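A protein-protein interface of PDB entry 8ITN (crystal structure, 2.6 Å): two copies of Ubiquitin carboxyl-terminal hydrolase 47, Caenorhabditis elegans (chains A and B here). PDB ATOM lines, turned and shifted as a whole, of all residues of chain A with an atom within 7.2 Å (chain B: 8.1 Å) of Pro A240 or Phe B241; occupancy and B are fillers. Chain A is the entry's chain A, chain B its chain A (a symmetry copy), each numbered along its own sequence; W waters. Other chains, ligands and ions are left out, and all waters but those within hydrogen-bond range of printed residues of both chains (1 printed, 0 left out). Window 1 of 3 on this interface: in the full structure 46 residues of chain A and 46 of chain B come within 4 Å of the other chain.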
ATOM      1  N   LEU A 234     -16.553 -23.079  22.688  1.00  0.00           N
ATOM      2  CA  LEU A 234     -15.313 -22.815  21.965  1.00  0.00           C
ATOM      3  C   LEU A 234     -14.533 -24.122  21.898  1.00  0.00           C
ATOM      4  O   LEU A 234     -13.754 -24.438  22.810  1.00  0.00           O
ATOM      5  CB  LEU A 234     -14.492 -21.715  22.640  1.00  0.00           C
ATOM      6  CG  LEU A 234     -13.933 -20.654  21.693  1.00  0.00           C
ATOM      7  CD1 LEU A 234     -15.021 -20.174  20.747  1.00  0.00           C
ATOM      8  CD2 LEU A 234     -13.343 -19.483  22.464  1.00  0.00           C
ATOM      9  N   PRO A 235     -14.726 -24.930  20.854  1.00  0.00           N
ATOM     10  CA  PRO A 235     -14.097 -26.257  20.810  1.00  0.00           C
ATOM     11  C   PRO A 235     -12.635 -26.202  20.395  1.00  0.00           C
ATOM     12  O   PRO A 235     -12.318 -26.173  19.202  1.00  0.00           O
ATOM     13  CB  PRO A 235     -14.947 -27.006  19.777  1.00  0.00           C
ATOM     14  CG  PRO A 235     -15.439 -25.929  18.859  1.00  0.00           C
ATOM     15  CD  PRO A 235     -15.596 -24.682  19.692  1.00  0.00           C
ATOM     16  N   LEU A 236     -11.736 -26.192  21.375  1.00  0.00           N
ATOM     17  CA  LEU A 236     -10.307 -26.079  21.125  1.00  0.00           C
ATOM     18  C   LEU A 236      -9.649 -27.444  21.267  1.00  0.00           C
ATOM     19  O   LEU A 236      -9.892 -28.159  22.246  1.00  0.00           O
ATOM     20  CB  LEU A 236      -9.663 -25.079  22.086  1.00  0.00           C
ATOM     21  CG  LEU A 236     -10.266 -23.674  22.065  1.00  0.00           C
ATOM     22  CD1 LEU A 236      -9.485 -22.737  22.973  1.00  0.00           C
ATOM     23  CD2 LEU A 236     -10.314 -23.138  20.643  1.00  0.00           C
ATOM     24  N   ALA A 237      -8.823 -27.801  20.290  1.00  0.00           N
ATOM     25  CA  ALA A 237      -8.077 -29.047  20.345  1.00  0.00           C
ATOM     26  C   ALA A 237      -6.833 -28.884  21.208  1.00  0.00           C
ATOM     27  O   ALA A 237      -6.294 -27.784  21.360  1.00  0.00           O
ATOM     28  CB  ALA A 237      -7.683 -29.500  18.940  1.00  0.00           C
ATOM     29  N   VAL A 238      -6.384 -29.995  21.780  1.00  0.00           N
ATOM     30  CA  VAL A 238      -5.149 -30.037  22.556  1.00  0.00           C
ATOM     31  C   VAL A 238      -3.976 -30.496  21.701  1.00  0.00           C
ATOM     32  O   VAL A 238      -2.945 -29.827  21.638  1.00  0.00           O
ATOM     33  CB  VAL A 238      -5.327 -30.938  23.798  1.00  0.00           C
ATOM     34  CG1 VAL A 238      -3.989 -31.171  24.478  1.00  0.00           C
ATOM     35  CG2 VAL A 238      -6.317 -30.310  24.765  1.00  0.00           C
ATOM     36  N   LYS A 239      -4.122 -31.638  21.035  1.00  0.00           N
ATOM     37  CA  LYS A 239      -3.116 -32.150  20.106  1.00  0.00           C
ATOM     38  C   LYS A 239      -3.819 -32.572  18.822  1.00  0.00           C
ATOM     39  O   LYS A 239      -4.421 -33.660  18.769  1.00  0.00           O
ATOM     40  CB  LYS A 239      -2.343 -33.318  20.704  1.00  0.00           C
ATOM     41  CG  LYS A 239      -1.190 -33.797  19.838  1.00  0.00           C
ATOM     42  CD  LYS A 239      -0.793 -35.225  20.175  1.00  0.00           C
ATOM     43  CE  LYS A 239      -1.805 -36.221  19.638  1.00  0.00           C
ATOM     44  NZ  LYS A 239      -1.857 -36.197  18.149  1.00  0.00           N
ATOM     45  N   PRO A 240      -3.776 -31.749  17.778  1.00  0.00           N
ATOM     46  CA  PRO A 240      -4.444 -32.111  16.525  1.00  0.00           C
ATOM     47  C   PRO A 240      -3.791 -33.316  15.864  1.00  0.00           C
ATOM     48  O   PRO A 240      -2.682 -33.731  16.207  1.00  0.00           O
ATOM     49  CB  PRO A 240      -4.285 -30.856  15.658  1.00  0.00           C
ATOM     50  CG  PRO A 240      -3.989 -29.751  16.624  1.00  0.00           C
ATOM     51  CD  PRO A 240      -3.213 -30.391  17.731  1.00  0.00           C
ATOM     52  N   PHE A 241      -4.517 -33.879  14.902  1.00  0.00           N
ATOM     53  CA  PHE A 241      -4.005 -34.997  14.121  1.00  0.00           C
ATOM     54  C   PHE A 241      -2.708 -34.601  13.425  1.00  0.00           C
ATOM     55  O   PHE A 241      -2.609 -33.520  12.836  1.00  0.00           O
ATOM     56  CB  PHE A 241      -5.056 -35.435  13.097  1.00  0.00           C
ATOM     57  CG  PHE A 241      -4.645 -36.611  12.253  1.00  0.00           C
ATOM     58  CD1 PHE A 241      -3.877 -36.432  11.111  1.00  0.00           C
ATOM     59  CD2 PHE A 241      -5.048 -37.894  12.586  1.00  0.00           C
ATOM     60  CE1 PHE A 241      -3.504 -37.509  10.332  1.00  0.00           C
ATOM     61  CE2 PHE A 241      -4.681 -38.975  11.807  1.00  0.00           C
ATOM     62  CZ  PHE A 241      -3.908 -38.781  10.678  1.00  0.00           C
ATOM     63  N   GLY A 242      -1.710 -35.478  13.500  1.00  0.00           N
ATOM     64  CA  GLY A 242      -0.439 -35.253  12.841  1.00  0.00           C
ATOM     65  C   GLY A 242       0.447 -34.200  13.466  1.00  0.00           C
ATOM     66  O   GLY A 242       1.553 -33.973  12.964  1.00  0.00           O
ATOM     67  N   ALA A 243       0.009 -33.556  14.545  1.00  0.00           N
ATOM     68  CA  ALA A 243       0.782 -32.475  15.141  1.00  0.00           C
ATOM     69  C   ALA A 243       2.046 -33.005  15.803  1.00  0.00           C
ATOM     70  O   ALA A 243       2.044 -34.069  16.431  1.00  0.00           O
ATOM     71  CB  ALA A 243      -0.066 -31.721  16.165  1.00  0.00           C
ATOM     72  N   ILE A 244       3.135 -32.254  15.658  1.00  0.00           N
ATOM     73  CA  ILE A 244       4.387 -32.594  16.326  1.00  0.00           C
ATOM     74  C   ILE A 244       4.420 -32.038  17.744  1.00  0.00           C
ATOM     75  O   ILE A 244       4.955 -32.673  18.655  1.00  0.00           O
ATOM     76  CB  ILE A 244       5.581 -32.093  15.488  1.00  0.00           C
ATOM     77  CG1 ILE A 244       5.641 -32.842  14.155  1.00  0.00           C
ATOM     78  CG2 ILE A 244       6.891 -32.256  16.251  1.00  0.00           C
ATOM     79  CD1 ILE A 244       6.859 -32.509  13.320  1.00  0.00           C
ATOM     80  N   HIS A 245       3.843 -30.859  17.952  1.00  0.00           N
ATOM     81  CA  HIS A 245       3.727 -30.259  19.272  1.00  0.00           C
ATOM     82  C   HIS A 245       2.260 -30.025  19.596  1.00  0.00           C
ATOM     83  O   HIS A 245       1.491 -29.575  18.741  1.00  0.00           O
ATOM     84  CB  HIS A 245       4.482 -28.931  19.353  1.00  0.00           C
ATOM     85  CG  HIS A 245       5.959 -29.061  19.158  1.00  0.00           C
ATOM     86  ND1 HIS A 245       6.830 -29.279  20.204  1.00  0.00           N
ATOM     87  CD2 HIS A 245       6.721 -28.996  18.041  1.00  0.00           C
ATOM     88  CE1 HIS A 245       8.064 -29.345  19.738  1.00  0.00           C
ATOM     89  NE2 HIS A 245       8.027 -29.177  18.429  1.00  0.00           N
ATOM     90  N   ALA A 246       1.876 -30.337  20.828  1.00  0.00           N
ATOM     91  CA  ALA A 246       0.551 -29.987  21.309  1.00  0.00           C
ATOM     92  C   ALA A 246       0.540 -28.538  21.776  1.00  0.00           C
ATOM     93  O   ALA A 246       1.572 -27.980  22.160  1.00  0.00           O
ATOM     94  CB  ALA A 246       0.125 -30.913  22.447  1.00  0.00           C
ATOM     95  N   TYR A 247      -0.639 -27.923  21.721  1.00  0.00           N
ATOM     96  CA  TYR A 247      -0.772 -26.536  22.141  1.00  0.00           C
ATOM     97  C   TYR A 247      -0.467 -26.407  23.627  1.00  0.00           C
ATOM     98  O   TYR A 247      -1.016 -27.138  24.455  1.00  0.00           O
ATOM     99  CB  TYR A 247      -2.179 -26.026  21.835  1.00  0.00           C
ATOM    100  CG  TYR A 247      -2.536 -26.094  20.367  1.00  0.00           C
ATOM    101  CD1 TYR A 247      -1.679 -25.586  19.400  1.00  0.00           C
ATOM    102  CD2 TYR A 247      -3.721 -26.683  19.947  1.00  0.00           C
ATOM    103  CE1 TYR A 247      -1.999 -25.652  18.056  1.00  0.00           C
ATOM    104  CE2 TYR A 247      -4.047 -26.756  18.608  1.00  0.00           C
ATOM    105  CZ  TYR A 247      -3.182 -26.239  17.667  1.00  0.00           C
ATOM    106  OH  TYR A 247      -3.503 -26.308  16.332  1.00  0.00           O
ATOM    107  N   GLU A 252      -3.064 -20.418  22.688  1.00  0.00           N
ATOM    108  CA  GLU A 252      -2.433 -20.920  21.471  1.00  0.00           C
ATOM    109  C   GLU A 252      -3.414 -21.743  20.643  1.00  0.00           C
ATOM    110  O   GLU A 252      -3.411 -21.667  19.409  1.00  0.00           O
ATOM    111  CB  GLU A 252      -1.197 -21.745  21.825  1.00  0.00           C
ATOM    112  CG  GLU A 252      -0.200 -21.891  20.690  1.00  0.00           C
ATOM    113  CD  GLU A 252       1.035 -22.670  21.100  1.00  0.00           C
ATOM    114  OE1 GLU A 252       0.889 -23.698  21.795  1.00  0.00           O
ATOM    115  OE2 GLU A 252       2.153 -22.249  20.736  1.00  0.00           O
ATOM    116  N   ALA A 253      -4.265 -22.529  21.307  1.00  0.00           N
ATOM    117  CA  ALA A 253      -5.264 -23.306  20.584  1.00  0.00           C
ATOM    118  C   ALA A 253      -6.335 -22.403  19.983  1.00  0.00           C
ATOM    119  O   ALA A 253      -6.835 -22.667  18.883  1.00  0.00           O
ATOM    120  CB  ALA A 253      -5.895 -24.344  21.511  1.00  0.00           C
ATOM    121  N   LEU A 254      -6.700 -21.331  20.691  1.00  0.00           N
ATOM    122  CA  LEU A 254      -7.679 -20.391  20.153  1.00  0.00           C
ATOM    123  C   LEU A 254      -7.115 -19.633  18.959  1.00  0.00           C
ATOM    124  O   LEU A 254      -7.845 -19.333  18.006  1.00  0.00           O
ATOM    125  CB  LEU A 254      -8.133 -19.422  21.244  1.00  0.00           C
ATOM    126  CG  LEU A 254      -9.183 -18.387  20.838  1.00  0.00           C
ATOM    127  CD1 LEU A 254     -10.412 -19.073  20.264  1.00  0.00           C
ATOM    128  CD2 LEU A 254      -9.558 -17.506  22.020  1.00  0.00           C
ATOM    129  N   THR A 255      -5.819 -19.315  18.989  1.00  0.00           N
ATOM    130  CA  THR A 255      -5.190 -18.662  17.845  1.00  0.00           C
ATOM    131  C   THR A 255      -5.217 -19.569  16.621  1.00  0.00           C
ATOM    132  O   THR A 255      -5.563 -19.134  15.516  1.00  0.00           O
ATOM    133  CB  THR A 255      -3.755 -18.263  18.193  1.00  0.00           C
ATOM    134  OG1 THR A 255      -3.766 -17.380  19.322  1.00  0.00           O
ATOM    135  CG2 THR A 255      -3.094 -17.563  17.014  1.00  0.00           C
ATOM    136  N   ALA A 256      -4.858 -20.842  16.802  1.00  0.00           N
ATOM    137  CA  ALA A 256      -4.969 -21.816  15.721  1.00  0.00           C
ATOM    138  C   ALA A 256      -6.415 -22.059  15.316  1.00  0.00           C
ATOM    139  O   ALA A 256      -6.668 -22.465  14.177  1.00  0.00           O
ATOM    140  CB  ALA A 256      -4.312 -23.134  16.135  1.00  0.00           C
ATOM    141  N   PHE A 257      -7.365 -21.820  16.222  1.00  0.00           N
ATOM    142  CA  PHE A 257      -8.775 -22.007  15.900  1.00  0.00           C
ATOM    143  C   PHE A 257      -9.263 -20.972  14.895  1.00  0.00           C
ATOM    144  O   PHE A 257     -10.128 -21.275  14.063  1.00  0.00           O
ATOM    145  CB  PHE A 257      -9.604 -21.952  17.185  1.00  0.00           C
ATOM    146  CG  PHE A 257     -11.086 -22.058  16.966  1.00  0.00           C
ATOM    147  CD1 PHE A 257     -11.657 -23.248  16.548  1.00  0.00           C
ATOM    148  CD2 PHE A 257     -11.909 -20.971  17.206  1.00  0.00           C
ATOM    149  CE1 PHE A 257     -13.023 -23.346  16.356  1.00  0.00           C
ATOM    150  CE2 PHE A 257     -13.274 -21.062  17.016  1.00  0.00           C
ATOM    151  CZ  PHE A 257     -13.832 -22.252  16.593  1.00  0.00           C
ATOM    152  N   VAL A 258      -8.721 -19.754  14.949  1.00  0.00           N
ATOM    153  CA  VAL A 258      -9.071 -18.704  14.000  1.00  0.00           C
ATOM    154  C   VAL A 258      -8.044 -18.591  12.876  1.00  0.00           C
ATOM    155  O   VAL A 258      -8.058 -17.609  12.127  1.00  0.00           O
ATOM    156  CB  VAL A 258      -9.256 -17.354  14.715  1.00  0.00           C
ATOM    157  CG1 VAL A 258     -10.306 -17.470  15.806  1.00  0.00           C
ATOM    158  CG2 VAL A 258      -7.935 -16.868  15.294  1.00  0.00           C
ATOM    159  N   LYS A 298     -10.392 -30.517  23.874  1.00  0.00           N
ATOM    160  CA  LYS A 298     -10.584 -31.816  23.226  1.00  0.00           C
ATOM    161  C   LYS A 298      -9.505 -32.810  23.662  1.00  0.00           C
ATOM    162  O   LYS A 298      -8.677 -33.273  22.878  1.00  0.00           O
ATOM    163  CB  LYS A 298     -10.604 -31.652  21.712  1.00  0.00           C
ATOM    164  CG  LYS A 298     -11.881 -31.038  21.164  1.00  0.00           C
ATOM    165  CD  LYS A 298     -11.652 -30.489  19.764  1.00  0.00           C
ATOM    166  CE  LYS A 298     -12.963 -30.206  19.052  1.00  0.00           C
ATOM    167  NZ  LYS A 298     -13.666 -31.464  18.677  1.00  0.00           N
ATOM    168  N   LEU A 312      -6.063 -37.403  25.890  1.00  0.00           N
ATOM    169  CA  LEU A 312      -4.726 -36.834  25.805  1.00  0.00           C
ATOM    170  C   LEU A 312      -4.329 -36.239  27.149  1.00  0.00           C
ATOM    171  O   LEU A 312      -5.158 -35.660  27.858  1.00  0.00           O
ATOM    172  CB  LEU A 312      -4.657 -35.756  24.722  1.00  0.00           C
ATOM    173  CG  LEU A 312      -4.710 -36.153  23.243  1.00  0.00           C
ATOM    174  CD1 LEU A 312      -3.834 -37.366  22.971  1.00  0.00           C
ATOM    175  CD2 LEU A 312      -6.138 -36.391  22.770  1.00  0.00           C
ATOM    176  N   ALA B 237      -7.273 -38.129   9.150  1.00  0.00           N
ATOM    177  CA  ALA B 237      -7.905 -36.824   9.056  1.00  0.00           C
ATOM    178  C   ALA B 237      -7.658 -36.212   7.683  1.00  0.00           C
ATOM    179  O   ALA B 237      -6.672 -36.521   7.008  1.00  0.00           O
ATOM    180  CB  ALA B 237      -7.376 -35.891  10.145  1.00  0.00           C
ATOM    181  N   VAL B 238      -8.574 -35.344   7.270  1.00  0.00           N
ATOM    182  CA  VAL B 238      -8.443 -34.593   6.027  1.00  0.00           C
ATOM    183  C   VAL B 238      -7.847 -33.215   6.275  1.00  0.00           C
ATOM    184  O   VAL B 238      -6.859 -32.836   5.648  1.00  0.00           O
ATOM    185  CB  VAL B 238      -9.810 -34.494   5.314  1.00  0.00           C
ATOM    186  CG1 VAL B 238      -9.729 -33.524   4.148  1.00  0.00           C
ATOM    187  CG2 VAL B 238     -10.255 -35.867   4.838  1.00  0.00           C
ATOM    188  N   LYS B 239      -8.438 -32.456   7.195  1.00  0.00           N
ATOM    189  CA  LYS B 239      -7.917 -31.151   7.601  1.00  0.00           C
ATOM    190  C   LYS B 239      -7.910 -31.090   9.123  1.00  0.00           C
ATOM    191  O   LYS B 239      -8.964 -30.863   9.743  1.00  0.00           O
ATOM    192  CB  LYS B 239      -8.746 -30.012   7.022  1.00  0.00           C
ATOM    193  CG  LYS B 239      -8.167 -28.633   7.295  1.00  0.00           C
ATOM    194  CD  LYS B 239      -9.228 -27.550   7.185  1.00  0.00           C
ATOM    195  CE  LYS B 239     -10.155 -27.561   8.387  1.00  0.00           C
ATOM    196  NZ  LYS B 239      -9.426 -27.233   9.643  1.00  0.00           N
ATOM    197  N   PRO B 240      -6.759 -31.294   9.758  1.00  0.00           N
ATOM    198  CA  PRO B 240      -6.707 -31.251  11.221  1.00  0.00           C
ATOM    199  C   PRO B 240      -6.994 -29.857  11.757  1.00  0.00           C
ATOM    200  O   PRO B 240      -6.984 -28.860  11.032  1.00  0.00           O
ATOM    201  CB  PRO B 240      -5.269 -31.677  11.542  1.00  0.00           C
ATOM    202  CG  PRO B 240      -4.787 -32.378  10.310  1.00  0.00           C
ATOM    203  CD  PRO B 240      -5.470 -31.690   9.170  1.00  0.00           C
ATOM    204  N   PHE B 241      -7.262 -29.809  13.060  1.00  0.00           N
ATOM    205  CA  PHE B 241      -7.487 -28.542  13.743  1.00  0.00           C
ATOM    206  C   PHE B 241      -6.273 -27.634  13.579  1.00  0.00           C
ATOM    207  O   PHE B 241      -5.130 -28.070  13.742  1.00  0.00           O
ATOM    208  CB  PHE B 241      -7.774 -28.799  15.225  1.00  0.00           C
ATOM    209  CG  PHE B 241      -8.056 -27.555  16.025  1.00  0.00           C
ATOM    210  CD1 PHE B 241      -7.018 -26.798  16.549  1.00  0.00           C
ATOM    211  CD2 PHE B 241      -9.359 -27.159  16.277  1.00  0.00           C
ATOM    212  CE1 PHE B 241      -7.275 -25.660  17.288  1.00  0.00           C
ATOM    213  CE2 PHE B 241      -9.622 -26.023  17.019  1.00  0.00           C
ATOM    214  CZ  PHE B 241      -8.578 -25.274  17.525  1.00  0.00           C
ATOM    215  N   GLY B 242      -6.526 -26.370  13.249  1.00  0.00           N
ATOM    216  CA  GLY B 242      -5.470 -25.387  13.111  1.00  0.00           C
ATOM    217  C   GLY B 242      -4.599 -25.528  11.884  1.00  0.00           C
ATOM    218  O   GLY B 242      -3.692 -24.709  11.697  1.00  0.00           O
ATOM    219  N   ALA B 243      -4.843 -26.525  11.039  1.00  0.00           N
ATOM    220  CA  ALA B 243      -3.986 -26.760   9.885  1.00  0.00           C
ATOM    221  C   ALA B 243      -4.152 -25.659   8.846  1.00  0.00           C
ATOM    222  O   ALA B 243      -5.259 -25.172   8.598  1.00  0.00           O
ATOM    223  CB  ALA B 243      -4.302 -28.118   9.259  1.00  0.00           C
ATOM    224  N   ILE B 244      -3.036 -25.266   8.236  1.00  0.00           N
ATOM    225  CA  ILE B 244      -3.067 -24.292   7.150  1.00  0.00           C
ATOM    226  C   ILE B 244      -3.336 -24.971   5.813  1.00  0.00           C
ATOM    227  O   ILE B 244      -4.026 -24.415   4.955  1.00  0.00           O
ATOM    228  CB  ILE B 244      -1.750 -23.488   7.128  1.00  0.00           C
ATOM    229  CG1 ILE B 244      -1.626 -22.644   8.399  1.00  0.00           C
ATOM    230  CG2 ILE B 244      -1.670 -22.604   5.890  1.00  0.00           C
ATOM    231  CD1 ILE B 244      -0.426 -21.721   8.405  1.00  0.00           C
ATOM    232  N   TYR B 247      -4.455 -32.293   3.951  1.00  0.00           N
ATOM    233  CA  TYR B 247      -3.682 -33.349   3.312  1.00  0.00           C
ATOM    234  C   TYR B 247      -4.185 -33.580   1.894  1.00  0.00           C
ATOM    235  O   TYR B 247      -5.384 -33.757   1.665  1.00  0.00           O
ATOM    236  CB  TYR B 247      -3.771 -34.635   4.131  1.00  0.00           C
ATOM    237  CG  TYR B 247      -3.255 -34.484   5.544  1.00  0.00           C
ATOM    238  CD1 TYR B 247      -2.018 -33.905   5.794  1.00  0.00           C
ATOM    239  CD2 TYR B 247      -4.013 -34.904   6.629  1.00  0.00           C
ATOM    240  CE1 TYR B 247      -1.546 -33.759   7.085  1.00  0.00           C
ATOM    241  CE2 TYR B 247      -3.549 -34.760   7.922  1.00  0.00           C
ATOM    242  CZ  TYR B 247      -2.315 -34.187   8.143  1.00  0.00           C
ATOM    243  OH  TYR B 247      -1.850 -34.043   9.429  1.00  0.00           O
ATOM    244  N   ALA B 256       1.412 -38.518   8.306  1.00  0.00           N
ATOM    245  CA  ALA B 256       1.168 -37.729   9.508  1.00  0.00           C
ATOM    246  C   ALA B 256       0.546 -38.560  10.623  1.00  0.00           C
ATOM    247  O   ALA B 256       0.693 -38.209  11.797  1.00  0.00           O
ATOM    248  CB  ALA B 256       0.267 -36.538   9.179  1.00  0.00           C
ATOM    249  N   GLN B 259       3.350 -39.970  12.490  1.00  0.00           N
ATOM    250  CA  GLN B 259       4.328 -38.940  12.830  1.00  0.00           C
ATOM    251  C   GLN B 259       4.531 -38.890  14.340  1.00  0.00           C
ATOM    252  O   GLN B 259       3.559 -38.729  15.086  1.00  0.00           O
ATOM    253  CB  GLN B 259       3.869 -37.574  12.321  1.00  0.00           C
ATOM    254  CG  GLN B 259       4.752 -36.418  12.763  1.00  0.00           C
ATOM    255  CD  GLN B 259       6.105 -36.428  12.086  1.00  0.00           C
ATOM    256  OE1 GLN B 259       6.235 -36.868  10.944  1.00  0.00           O
ATOM    257  NE2 GLN B 259       7.124 -35.945  12.789  1.00  0.00           N
ATOM    258  N   GLU B 261       4.979 -37.481  17.879  1.00  0.00           N
ATOM    259  CA  GLU B 261       4.823 -36.227  18.602  1.00  0.00           C
ATOM    260  C   GLU B 261       6.046 -35.979  19.475  1.00  0.00           C
ATOM    261  O   GLU B 261       6.553 -36.891  20.132  1.00  0.00           O
ATOM    262  CB  GLU B 261       3.563 -36.254  19.468  1.00  0.00           C
ATOM    263  CG  GLU B 261       3.319 -34.964  20.231  1.00  0.00           C
ATOM    264  CD  GLU B 261       2.359 -35.139  21.392  1.00  0.00           C
ATOM    265  OE1 GLU B 261       2.009 -36.295  21.712  1.00  0.00           O
ATOM    266  OE2 GLU B 261       1.953 -34.118  21.985  1.00  0.00           O
ATOM    267  N   ASP B 301     -17.591 -34.324  10.592  1.00  0.00           N
ATOM    268  CA  ASP B 301     -17.494 -33.950  11.992  1.00  0.00           C
ATOM    269  C   ASP B 301     -18.891 -33.609  12.490  1.00  0.00           C
ATOM    270  O   ASP B 301     -19.824 -33.428  11.702  1.00  0.00           O
ATOM    271  CB  ASP B 301     -16.540 -32.764  12.185  1.00  0.00           C
ATOM    272  CG  ASP B 301     -15.907 -32.740  13.562  1.00  0.00           C
ATOM    273  OD1 ASP B 301     -16.173 -33.665  14.359  1.00  0.00           O
ATOM    274  OD2 ASP B 301     -15.137 -31.796  13.845  1.00  0.00           O
HETATM  275  O   HOH W   1       3.706 -31.403  22.726  1.00  0.00           O
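The backbone carbonyl oxygen (O) of Val B238 is in hydrogen-bond range of the backbone NH (N) of Tyr B247.
The backbone NH of Tyr A247 sits at hydrogen-bond distance from the backbone carbonyl oxygen of Val A238 (3.0 Å).
Among the printed residues, merely in contact across the chains: Ile A244 with Glu B261, Gly A242 with Ala B256, Ala A256 with Gly B242, Lys A239 with Glu B261, Ala A253 with Phe B241, Pro A235 with Phe B241, Phe A257 with Phe B241, Phe A241 with Pro B240, Pro A240 with Phe B241, Ile A244 with Gln B259, Ala A237 with Phe B241, Phe A241 with Ala B237, Phe A241 with Tyr B247, Tyr A247 with Phe B241, Ala A246 with Glu B261, Tyr A247 with Gly B242 and Gly A242 with Tyr B247.
Phe B241 touches just these residues of chain A: Pro A235 (3.5 Å), Ala A237 (3.5 Å), Pro A240 (3.5 Å), Tyr A247 (3.5 Å), Ala A253 (3.4 Å) and Phe A257 (3.5 Å).
Of the printed residues of chain A, Gly B242 touches Tyr A247 (3.9 Å) and Ala A256 (3.3 Å).
Of the printed residues of chain B, Ala A246 touches Glu B261 (3.7 Å).
Of the printed residues of chain B, Phe A257 touches Phe B241 (3.5 Å).
Printed residues of chain B within 4 Å of Lys A239: Glu B261.
The nearest printed residue of chain A that does not touch Phe B241 is Ala A256 (4.1 Å).
Hydrophobic or aromatic side chains of chain A that line the printed part of chain B: Ala A237, Pro A240, Phe A241, Ile A244, Ala A246, Tyr A247, Ala A256 and Phe A257.
Among the printed residues, 17 pairs touch across the chains.
Ala A237 touches Phe B241, and with the chains exchanged Phe A241 touches Ala B237.
Pro A240 touches Phe B241, and with the chains exchanged Phe A241 touches Pro B240.
Phe A241 touches Tyr B247, and with the chains exchanged Tyr A247 touches Phe B241.
Gly A242 touches Tyr B247, and with the chains exchanged Tyr A247 touches Gly B242.
10 positions are printed for both chains.
Water W1 bridges the backbone NH (N) of Ala A246 and the side-chain carboxylate (OE2) of Glu B261.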
